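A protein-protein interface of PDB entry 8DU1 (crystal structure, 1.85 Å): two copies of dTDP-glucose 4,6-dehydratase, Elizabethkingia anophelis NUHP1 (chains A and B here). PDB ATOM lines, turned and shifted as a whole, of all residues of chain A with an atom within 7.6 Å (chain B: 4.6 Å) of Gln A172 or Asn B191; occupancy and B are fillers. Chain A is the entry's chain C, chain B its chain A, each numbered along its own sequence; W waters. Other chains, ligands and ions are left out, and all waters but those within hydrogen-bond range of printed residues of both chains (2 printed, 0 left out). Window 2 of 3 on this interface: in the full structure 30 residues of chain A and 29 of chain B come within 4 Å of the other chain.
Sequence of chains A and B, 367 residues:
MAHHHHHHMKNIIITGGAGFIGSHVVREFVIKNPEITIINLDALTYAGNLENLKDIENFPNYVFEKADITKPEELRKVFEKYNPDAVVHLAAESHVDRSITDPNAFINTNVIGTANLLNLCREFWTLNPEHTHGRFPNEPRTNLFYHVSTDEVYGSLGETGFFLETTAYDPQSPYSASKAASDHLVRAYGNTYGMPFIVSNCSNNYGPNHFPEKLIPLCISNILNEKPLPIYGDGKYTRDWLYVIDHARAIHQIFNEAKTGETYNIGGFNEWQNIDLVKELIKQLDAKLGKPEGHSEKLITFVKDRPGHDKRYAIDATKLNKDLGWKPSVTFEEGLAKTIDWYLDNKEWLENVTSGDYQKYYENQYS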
ATOM      1  N   GLU A 152     -20.011  24.196  20.823  1.00  0.00           N
ATOM      2  CA  GLU A 152     -20.089  24.323  19.366  1.00  0.00           C
ATOM      3  C   GLU A 152     -18.837  23.830  18.658  1.00  0.00           C
ATOM      4  O   GLU A 152     -18.859  23.690  17.429  1.00  0.00           O
ATOM      5  CB  GLU A 152     -20.348  25.773  18.966  1.00  0.00           C
ATOM      6  CG  GLU A 152     -21.675  26.342  19.482  1.00  0.00           C
ATOM      7  CD  GLU A 152     -21.871  27.779  19.028  1.00  0.00           C
ATOM      8  OE1 GLU A 152     -21.724  28.041  17.815  1.00  0.00           O
ATOM      9  OE2 GLU A 152     -22.150  28.648  19.881  1.00  0.00           O
ATOM     10  N   VAL A 153     -17.745  23.589  19.385  1.00  0.00           N
ATOM     11  CA  VAL A 153     -16.580  22.975  18.748  1.00  0.00           C
ATOM     12  C   VAL A 153     -16.920  21.599  18.187  1.00  0.00           C
ATOM     13  O   VAL A 153     -16.236  21.119  17.273  1.00  0.00           O
ATOM     14  CB  VAL A 153     -15.387  22.867  19.729  1.00  0.00           C
ATOM     15  CG1 VAL A 153     -14.984  24.243  20.296  1.00  0.00           C
ATOM     16  CG2 VAL A 153     -15.693  21.864  20.852  1.00  0.00           C
ATOM     17  N   TYR A 154     -17.954  20.941  18.716  1.00  0.00           N
ATOM     18  CA  TYR A 154     -18.298  19.584  18.304  1.00  0.00           C
ATOM     19  C   TYR A 154     -19.199  19.526  17.081  1.00  0.00           C
ATOM     20  O   TYR A 154     -19.533  18.426  16.625  1.00  0.00           O
ATOM     21  CB  TYR A 154     -18.996  18.847  19.443  1.00  0.00           C
ATOM     22  CG  TYR A 154     -18.160  18.667  20.685  1.00  0.00           C
ATOM     23  CD1 TYR A 154     -17.018  17.876  20.669  1.00  0.00           C
ATOM     24  CD2 TYR A 154     -18.555  19.242  21.892  1.00  0.00           C
ATOM     25  CE1 TYR A 154     -16.271  17.692  21.798  1.00  0.00           C
ATOM     26  CE2 TYR A 154     -17.824  19.060  23.031  1.00  0.00           C
ATOM     27  CZ  TYR A 154     -16.681  18.285  22.980  1.00  0.00           C
ATOM     28  OH  TYR A 154     -15.959  18.102  24.126  1.00  0.00           O
ATOM     29  N   GLY A 155     -19.626  20.658  16.560  1.00  0.00           N
ATOM     30  CA  GLY A 155     -20.512  20.660  15.410  1.00  0.00           C
ATOM     31  C   GLY A 155     -21.953  20.562  15.849  1.00  0.00           C
ATOM     32  O   GLY A 155     -22.381  21.293  16.734  1.00  0.00           O
ATOM     33  N   SER A 156     -22.699  19.649  15.230  1.00  0.00           N
ATOM     34  CA  SER A 156     -24.125  19.510  15.492  1.00  0.00           C
ATOM     35  C   SER A 156     -24.480  18.033  15.462  1.00  0.00           C
ATOM     36  O   SER A 156     -23.684  17.186  15.041  1.00  0.00           O
ATOM     37  CB  SER A 156     -24.970  20.297  14.477  1.00  0.00           C
ATOM     38  OG  SER A 156     -24.759  19.798  13.165  1.00  0.00           O
ATOM     39  N   LEU A 157     -25.696  17.730  15.905  1.00  0.00           N
ATOM     40  CA  LEU A 157     -26.159  16.362  16.048  1.00  0.00           C
ATOM     41  C   LEU A 157     -27.363  16.111  15.154  1.00  0.00           C
ATOM     42  O   LEU A 157     -28.100  17.037  14.797  1.00  0.00           O
ATOM     43  CB  LEU A 157     -26.531  16.062  17.517  1.00  0.00           C
ATOM     44  CG  LEU A 157     -25.406  16.262  18.535  1.00  0.00           C
ATOM     45  CD1 LEU A 157     -25.951  16.286  19.968  1.00  0.00           C
ATOM     46  CD2 LEU A 157     -24.354  15.176  18.386  1.00  0.00           C
ATOM     47  N   PHE A 163     -22.963  15.311  22.471  1.00  0.00           N
ATOM     48  CA  PHE A 163     -21.552  15.689  22.469  1.00  0.00           C
ATOM     49  C   PHE A 163     -20.847  15.059  23.666  1.00  0.00           C
ATOM     50  O   PHE A 163     -21.218  15.310  24.818  1.00  0.00           O
ATOM     51  CB  PHE A 163     -21.373  17.204  22.541  1.00  0.00           C
ATOM     52  CG  PHE A 163     -22.048  17.982  21.447  1.00  0.00           C
ATOM     53  CD1 PHE A 163     -21.993  17.567  20.122  1.00  0.00           C
ATOM     54  CD2 PHE A 163     -22.717  19.153  21.753  1.00  0.00           C
ATOM     55  CE1 PHE A 163     -22.587  18.314  19.132  1.00  0.00           C
ATOM     56  CE2 PHE A 163     -23.322  19.903  20.766  1.00  0.00           C
ATOM     57  CZ  PHE A 163     -23.254  19.487  19.452  1.00  0.00           C
ATOM     58  N   TYR A 169     -14.022  17.118  16.908  1.00  0.00           N
ATOM     59  CA  TYR A 169     -14.319  18.513  16.603  1.00  0.00           C
ATOM     60  C   TYR A 169     -14.869  18.644  15.195  1.00  0.00           C
ATOM     61  O   TYR A 169     -14.379  18.008  14.257  1.00  0.00           O
ATOM     62  CB  TYR A 169     -13.062  19.383  16.727  1.00  0.00           C
ATOM     63  CG  TYR A 169     -12.735  19.866  18.120  1.00  0.00           C
ATOM     64  CD1 TYR A 169     -13.194  19.182  19.245  1.00  0.00           C
ATOM     65  CD2 TYR A 169     -11.960  21.011  18.309  1.00  0.00           C
ATOM     66  CE1 TYR A 169     -12.896  19.622  20.526  1.00  0.00           C
ATOM     67  CE2 TYR A 169     -11.663  21.467  19.590  1.00  0.00           C
ATOM     68  CZ  TYR A 169     -12.128  20.756  20.687  1.00  0.00           C
ATOM     69  OH  TYR A 169     -11.832  21.184  21.948  1.00  0.00           O
ATOM     70  N   ASP A 170     -15.891  19.498  15.044  1.00  0.00           N
ATOM     71  CA  ASP A 170     -16.480  19.778  13.740  1.00  0.00           C
ATOM     72  C   ASP A 170     -17.166  21.142  13.772  1.00  0.00           C
ATOM     73  O   ASP A 170     -18.361  21.253  13.452  1.00  0.00           O
ATOM     74  CB  ASP A 170     -17.445  18.653  13.346  1.00  0.00           C
ATOM     75  CG  ASP A 170     -18.053  18.850  11.972  1.00  0.00           C
ATOM     76  OD1 ASP A 170     -17.410  19.460  11.093  1.00  0.00           O
ATOM     77  OD2 ASP A 170     -19.199  18.408  11.782  1.00  0.00           O
ATOM     78  N   PRO A 171     -16.437  22.210  14.107  1.00  0.00           N
ATOM     79  CA  PRO A 171     -17.075  23.531  14.240  1.00  0.00           C
ATOM     80  C   PRO A 171     -17.642  24.007  12.908  1.00  0.00           C
ATOM     81  O   PRO A 171     -17.015  23.869  11.859  1.00  0.00           O
ATOM     82  CB  PRO A 171     -15.931  24.431  14.719  1.00  0.00           C
ATOM     83  CG  PRO A 171     -14.676  23.753  14.131  1.00  0.00           C
ATOM     84  CD  PRO A 171     -14.964  22.284  14.196  1.00  0.00           C
ATOM     85  N   GLN A 172     -18.844  24.576  12.954  1.00  0.00           N
ATOM     86  CA  GLN A 172     -19.588  24.862  11.738  1.00  0.00           C
ATOM     87  C   GLN A 172     -19.729  26.350  11.461  1.00  0.00           C
ATOM     88  O   GLN A 172     -20.225  26.726  10.390  1.00  0.00           O
ATOM     89  CB  GLN A 172     -20.968  24.186  11.798  1.00  0.00           C
ATOM     90  CG  GLN A 172     -20.861  22.677  11.598  1.00  0.00           C
ATOM     91  CD  GLN A 172     -22.087  21.940  12.082  1.00  0.00           C
ATOM     92  OE1 GLN A 172     -23.005  22.542  12.631  1.00  0.00           O
ATOM     93  NE2 GLN A 172     -22.100  20.628  11.898  1.00  0.00           N
ATOM     94  N   SER A 173     -19.272  27.200  12.366  1.00  0.00           N
ATOM     95  CA  SER A 173     -19.336  28.639  12.186  1.00  0.00           C
ATOM     96  C   SER A 173     -17.953  29.236  12.382  1.00  0.00           C
ATOM     97  O   SER A 173     -17.087  28.635  13.032  1.00  0.00           O
ATOM     98  CB  SER A 173     -20.325  29.274  13.175  1.00  0.00           C
ATOM     99  OG  SER A 173     -19.834  29.206  14.504  1.00  0.00           O
ATOM    100  N   PRO A 174     -17.701  30.405  11.808  1.00  0.00           N
ATOM    101  CA  PRO A 174     -16.418  31.073  12.066  1.00  0.00           C
ATOM    102  C   PRO A 174     -16.133  31.248  13.548  1.00  0.00           C
ATOM    103  O   PRO A 174     -15.000  31.019  13.987  1.00  0.00           O
ATOM    104  CB  PRO A 174     -16.578  32.414  11.334  1.00  0.00           C
ATOM    105  CG  PRO A 174     -17.518  32.092  10.204  1.00  0.00           C
ATOM    106  CD  PRO A 174     -18.499  31.098  10.781  1.00  0.00           C
ATOM    107  N   TYR A 175     -17.140  31.627  14.339  1.00  0.00           N
ATOM    108  CA  TYR A 175     -16.928  31.753  15.774  1.00  0.00           C
ATOM    109  C   TYR A 175     -16.452  30.437  16.367  1.00  0.00           C
ATOM    110  O   TYR A 175     -15.426  30.388  17.051  1.00  0.00           O
ATOM    111  CB  TYR A 175     -18.219  32.214  16.465  1.00  0.00           C
ATOM    112  CG  TYR A 175     -18.181  32.098  17.974  1.00  0.00           C
ATOM    113  CD1 TYR A 175     -17.369  32.929  18.727  1.00  0.00           C
ATOM    114  CD2 TYR A 175     -18.964  31.163  18.644  1.00  0.00           C
ATOM    115  CE1 TYR A 175     -17.321  32.835  20.096  1.00  0.00           C
ATOM    116  CE2 TYR A 175     -18.925  31.063  20.030  1.00  0.00           C
ATOM    117  CZ  TYR A 175     -18.099  31.912  20.747  1.00  0.00           C
ATOM    118  OH  TYR A 175     -18.039  31.845  22.128  1.00  0.00           O
ATOM    119  N   SER A 176     -17.193  29.355  16.116  1.00  0.00           N
ATOM    120  CA  SER A 176     -16.865  28.105  16.784  1.00  0.00           C
ATOM    121  C   SER A 176     -15.560  27.533  16.240  1.00  0.00           C
ATOM    122  O   SER A 176     -14.835  26.848  16.974  1.00  0.00           O
ATOM    123  CB  SER A 176     -18.027  27.104  16.672  1.00  0.00           C
ATOM    124  OG  SER A 176     -18.289  26.677  15.338  1.00  0.00           O
ATOM    125  N   ALA A 177     -15.213  27.842  14.987  1.00  0.00           N
ATOM    126  CA  ALA A 177     -13.879  27.465  14.502  1.00  0.00           C
ATOM    127  C   ALA A 177     -12.788  28.199  15.280  1.00  0.00           C
ATOM    128  O   ALA A 177     -11.767  27.607  15.648  1.00  0.00           O
ATOM    129  CB  ALA A 177     -13.765  27.744  13.005  1.00  0.00           C
ATOM    130  N   PRO A 307     -32.224  27.903   7.087  1.00  0.00           N
ATOM    131  CA  PRO A 307     -31.411  26.752   6.684  1.00  0.00           C
ATOM    132  C   PRO A 307     -30.558  26.285   7.851  1.00  0.00           C
ATOM    133  O   PRO A 307     -29.872  27.079   8.497  1.00  0.00           O
ATOM    134  CB  PRO A 307     -30.557  27.303   5.536  1.00  0.00           C
ATOM    135  CG  PRO A 307     -31.320  28.487   5.028  1.00  0.00           C
ATOM    136  CD  PRO A 307     -31.961  29.083   6.248  1.00  0.00           C
ATOM    137  N   GLY A 308     -30.624  24.987   8.136  1.00  0.00           N
ATOM    138  CA  GLY A 308     -29.922  24.433   9.271  1.00  0.00           C
ATOM    139  C   GLY A 308     -30.575  24.671  10.615  1.00  0.00           C
ATOM    140  O   GLY A 308     -30.004  24.274  11.639  1.00  0.00           O
ATOM    141  N   LYS A 311     -31.382  21.722  13.578  1.00  0.00           N
ATOM    142  CA  LYS A 311     -30.150  21.243  14.180  1.00  0.00           C
ATOM    143  C   LYS A 311     -30.365  20.956  15.661  1.00  0.00           C
ATOM    144  O   LYS A 311     -31.273  21.491  16.301  1.00  0.00           O
ATOM    145  CB  LYS A 311     -29.010  22.259  13.999  1.00  0.00           C
ATOM    146  N   ARG A 312     -29.506  20.100  16.200  1.00  0.00           N
ATOM    147  CA  ARG A 312     -29.606  19.666  17.583  1.00  0.00           C
ATOM    148  C   ARG A 312     -28.235  19.762  18.230  1.00  0.00           C
ATOM    149  O   ARG A 312     -27.246  19.284  17.667  1.00  0.00           O
ATOM    150  CB  ARG A 312     -30.152  18.240  17.653  1.00  0.00           C
ATOM    151  CG  ARG A 312     -30.220  17.657  19.039  1.00  0.00           C
ATOM    152  CD  ARG A 312     -31.073  16.381  19.053  1.00  0.00           C
ATOM    153  NE  ARG A 312     -30.856  15.673  20.307  1.00  0.00           N
ATOM    154  CZ  ARG A 312     -29.890  14.784  20.493  1.00  0.00           C
ATOM    155  NH1 ARG A 312     -29.118  14.384  19.490  1.00  0.00           N
ATOM    156  NH2 ARG A 312     -29.691  14.291  21.711  1.00  0.00           N
ATOM    157  N   TYR A 313     -28.180  20.397  19.397  1.00  0.00           N
ATOM    158  CA  TYR A 313     -26.943  20.613  20.142  1.00  0.00           C
ATOM    159  C   TYR A 313     -27.231  20.168  21.568  1.00  0.00           C
ATOM    160  O   TYR A 313     -27.920  20.874  22.310  1.00  0.00           O
ATOM    161  CB  TYR A 313     -26.494  22.074  20.102  1.00  0.00           C
ATOM    162  CG  TYR A 313     -26.379  22.637  18.711  1.00  0.00           C
ATOM    163  CD1 TYR A 313     -27.503  23.083  18.028  1.00  0.00           C
ATOM    164  CD2 TYR A 313     -25.148  22.720  18.071  1.00  0.00           C
ATOM    165  CE1 TYR A 313     -27.408  23.594  16.745  1.00  0.00           C
ATOM    166  CE2 TYR A 313     -25.042  23.230  16.779  1.00  0.00           C
ATOM    167  CZ  TYR A 313     -26.174  23.665  16.126  1.00  0.00           C
ATOM    168  OH  TYR A 313     -26.079  24.173  14.847  1.00  0.00           O
ATOM    169  N   THR B 132     -25.492  26.555   1.581  1.00  0.00           N
ATOM    170  CA  THR B 132     -24.969  26.518   2.935  1.00  0.00           C
ATOM    171  C   THR B 132     -25.425  25.241   3.634  1.00  0.00           C
ATOM    172  O   THR B 132     -26.276  24.495   3.141  1.00  0.00           O
ATOM    173  CB  THR B 132     -25.425  27.743   3.722  1.00  0.00           C
ATOM    174  OG1 THR B 132     -26.831  27.637   3.964  1.00  0.00           O
ATOM    175  CG2 THR B 132     -25.131  29.019   2.928  1.00  0.00           C
ATOM    176  N   HIS B 133     -24.836  24.989   4.798  1.00  0.00           N
ATOM    177  CA  HIS B 133     -25.180  23.824   5.607  1.00  0.00           C
ATOM    178  C   HIS B 133     -25.076  22.529   4.807  1.00  0.00           C
ATOM    179  O   HIS B 133     -25.925  21.642   4.906  1.00  0.00           O
ATOM    180  CB  HIS B 133     -26.561  23.992   6.222  1.00  0.00           C
ATOM    181  CG  HIS B 133     -26.627  25.131   7.183  1.00  0.00           C
ATOM    182  ND1 HIS B 133     -26.887  26.425   6.785  1.00  0.00           N
ATOM    183  CD2 HIS B 133     -26.403  25.184   8.517  1.00  0.00           C
ATOM    184  CE1 HIS B 133     -26.855  27.220   7.840  1.00  0.00           C
ATOM    185  NE2 HIS B 133     -26.561  26.492   8.903  1.00  0.00           N
ATOM    186  N   GLY B 134     -24.020  22.432   4.001  1.00  0.00           N
ATOM    187  CA  GLY B 134     -23.702  21.200   3.312  1.00  0.00           C
ATOM    188  C   GLY B 134     -24.598  20.858   2.148  1.00  0.00           C
ATOM    189  O   GLY B 134     -24.700  19.682   1.787  1.00  0.00           O
ATOM    190  N   ARG B 187     -13.679  24.750   6.712  1.00  0.00           N
ATOM    191  CA  ARG B 187     -14.954  24.039   6.773  1.00  0.00           C
ATOM    192  C   ARG B 187     -16.085  24.949   7.240  1.00  0.00           C
ATOM    193  O   ARG B 187     -17.217  24.848   6.749  1.00  0.00           O
ATOM    194  CB  ARG B 187     -14.843  22.825   7.687  1.00  0.00           C
ATOM    195  CG  ARG B 187     -13.858  21.782   7.152  1.00  0.00           C
ATOM    196  CD  ARG B 187     -14.202  20.410   7.680  1.00  0.00           C
ATOM    197  NE  ARG B 187     -13.261  19.414   7.172  1.00  0.00           N
ATOM    198  CZ  ARG B 187     -12.114  19.106   7.757  1.00  0.00           C
ATOM    199  NH1 ARG B 187     -11.694  19.747   8.838  1.00  0.00           N
ATOM    200  NH2 ARG B 187     -11.356  18.152   7.230  1.00  0.00           N
ATOM    201  N   ALA B 188     -15.798  25.846   8.181  1.00  0.00           N
ATOM    202  CA  ALA B 188     -16.850  26.725   8.689  1.00  0.00           C
ATOM    203  C   ALA B 188     -17.280  27.746   7.642  1.00  0.00           C
ATOM    204  O   ALA B 188     -18.463  28.081   7.555  1.00  0.00           O
ATOM    205  CB  ALA B 188     -16.384  27.430   9.958  1.00  0.00           C
ATOM    206  N   TYR B 189     -16.343  28.268   6.845  1.00  0.00           N
ATOM    207  CA  TYR B 189     -16.754  29.139   5.744  1.00  0.00           C
ATOM    208  C   TYR B 189     -17.560  28.355   4.715  1.00  0.00           C
ATOM    209  O   TYR B 189     -18.540  28.862   4.163  1.00  0.00           O
ATOM    210  CB  TYR B 189     -15.534  29.788   5.083  1.00  0.00           C
ATOM    211  CG  TYR B 189     -15.004  31.021   5.785  1.00  0.00           C
ATOM    212  CD1 TYR B 189     -14.694  31.001   7.140  1.00  0.00           C
ATOM    213  CD2 TYR B 189     -14.777  32.199   5.075  1.00  0.00           C
ATOM    214  CE1 TYR B 189     -14.190  32.128   7.780  1.00  0.00           C
ATOM    215  CE2 TYR B 189     -14.278  33.332   5.703  1.00  0.00           C
ATOM    216  CZ  TYR B 189     -13.983  33.287   7.052  1.00  0.00           C
ATOM    217  OH  TYR B 189     -13.478  34.407   7.660  1.00  0.00           O
ATOM    218  N   GLY B 190     -17.164  27.110   4.453  1.00  0.00           N
ATOM    219  CA  GLY B 190     -17.957  26.270   3.575  1.00  0.00           C
ATOM    220  C   GLY B 190     -19.375  26.087   4.076  1.00  0.00           C
ATOM    221  O   GLY B 190     -20.341  26.256   3.327  1.00  0.00           O
ATOM    222  N   ASN B 191     -19.520  25.744   5.358  1.00  0.00           N
ATOM    223  CA  ASN B 191     -20.852  25.522   5.913  1.00  0.00           C
ATOM    224  C   ASN B 191     -21.652  26.818   5.974  1.00  0.00           C
ATOM    225  O   ASN B 191     -22.836  26.840   5.627  1.00  0.00           O
ATOM    226  CB  ASN B 191     -20.748  24.927   7.312  1.00  0.00           C
ATOM    227  CG  ASN B 191     -22.103  24.629   7.913  1.00  0.00           C
ATOM    228  OD1 ASN B 191     -22.782  23.719   7.468  1.00  0.00           O
ATOM    229  ND2 ASN B 191     -22.501  25.388   8.929  1.00  0.00           N
ATOM    230  N   THR B 192     -21.029  27.896   6.444  1.00  0.00           N
ATOM    231  CA  THR B 192     -21.777  29.107   6.770  1.00  0.00           C
ATOM    232  C   THR B 192     -22.101  29.939   5.539  1.00  0.00           C
ATOM    233  O   THR B 192     -23.165  30.563   5.471  1.00  0.00           O
ATOM    234  CB  THR B 192     -20.984  29.951   7.764  1.00  0.00           C
ATOM    235  OG1 THR B 192     -20.749  29.189   8.949  1.00  0.00           O
ATOM    236  CG2 THR B 192     -21.751  31.214   8.134  1.00  0.00           C
ATOM    237  N   TYR B 193     -21.197  29.983   4.567  1.00  0.00           N
ATOM    238  CA  TYR B 193     -21.375  30.832   3.399  1.00  0.00           C
ATOM    239  C   TYR B 193     -21.603  30.041   2.124  1.00  0.00           C
ATOM    240  O   TYR B 193     -21.884  30.647   1.082  1.00  0.00           O
ATOM    241  CB  TYR B 193     -20.160  31.757   3.223  1.00  0.00           C
ATOM    242  CG  TYR B 193     -19.809  32.502   4.491  1.00  0.00           C
ATOM    243  CD1 TYR B 193     -20.714  33.401   5.052  1.00  0.00           C
ATOM    244  CD2 TYR B 193     -18.593  32.302   5.132  1.00  0.00           C
ATOM    245  CE1 TYR B 193     -20.422  34.079   6.212  1.00  0.00           C
ATOM    246  CE2 TYR B 193     -18.288  32.985   6.307  1.00  0.00           C
ATOM    247  CZ  TYR B 193     -19.214  33.867   6.838  1.00  0.00           C
ATOM    248  OH  TYR B 193     -18.931  34.547   7.994  1.00  0.00           O
ATOM    249  N   GLY B 194     -21.503  28.714   2.177  1.00  0.00           N
ATOM    250  CA  GLY B 194     -21.650  27.927   0.972  1.00  0.00           C
ATOM    251  C   GLY B 194     -20.433  27.990   0.085  1.00  0.00           C
ATOM    252  O   GLY B 194     -20.545  27.816  -1.137  1.00  0.00           O
HETATM  253  O   HOH W   1     -22.807  28.710  10.718  1.00  0.00           O
HETATM  254  O   HOH W   2     -13.021  18.590  11.788  1.00  0.00           O
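NE2 of His B133 sits close to O of Pro A307, 3.4 Å away. The side-chain amide nitrogen of Asn B191 lies within hydrogen-bond range of the backbone carbonyl oxygen of Gln A172 (3.0 Å). The backbone carbonyl oxygen (O) of Gln A172 is in hydrogen-bond range of the side-chain hydroxyl (OG1) of Thr B192 (2.9 Å).
A ring nitrogen (ND1) of His B133 sits at hydrogen-bond distance from the side-chain hydroxyl of Thr B132 (3.1 Å). The backbone carbonyl oxygen of Asn B191 is in hydrogen-bond range of the backbone NH of His B133, at 2.8 Å. The backbone carbonyl oxygen (O) of Ala B188 is in hydrogen-bond range of the side-chain hydroxyl (OG1) of Thr B192, at 2.9 Å. The side-chain amide nitrogen of Gln A172 is in hydrogen-bond range of the side-chain hydroxyl of Ser A156, at 3.1 Å. The backbone NH (N) of Gln A172 is in hydrogen-bond range of the side-chain hydroxyl (OG) of Ser A176 (3.2 Å). The side-chain hydroxyl (OG) of Ser A176 sits at hydrogen-bond distance from the side-chain hydroxyl (OG) of Ser A173 (3.1 Å).
Ala B188 touches Gln A172. Ser A173 touches Ala B188. Ser A173 touches Thr B192. CB of Ala B188 touches N of Pro A174 (3.7 Å). CD of Pro A174 touches OG1 of Thr B192, at 3.5 Å. Tyr B193 touches Pro A174. His B133 touches Gly A308.
Val A153 touches none of the printed residues of chain B. Leu A157 touches none of the printed residues of chain B. Of the printed residues of chain B, Gln A172 touches Ala B188, Asn B191 and Thr B192. Printed residues of chain B within 4 Å of Ser A173: Ala B188 and Thr B192. Of the printed residues of chain B, Gly A308 touches His B133. Printed residues of chain A within 4 Å of His B133: Pro A307 (3.1 Å) and Gly A308 (3.7 Å). Asn B191 touches just one residue of chain A: Gln A172. Of the printed residues of chain A, Thr B192 touches Gln A172, Ser A173 and Pro A174. Printed residues of chain A within 4 Å of Tyr B193: Pro A174 (3.6 Å). The nearest printed residue of chain B that does not touch Gln A172 is Arg B187 (5.1 Å).
Printed residues of chain B that touch a printed residue of chain A: His B133, Ala B188, Asn B191, Thr B192 and Tyr B193. Among the printed residues, no Asp or Glu carboxylate lies within 4 Å of a Lys or Arg side-chain nitrogen of the other chain.
No position is printed for both chains.
Water W1 bridges OG1 of Thr B192 (2.8 Å) and O of Gln A172 (3.3 Å). Water W2 lies within hydrogen-bond range of the backbone carbonyl oxygen of Tyr A169 (2.9 Å) and the guanidinium group of Arg B187 (3.4 Å).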
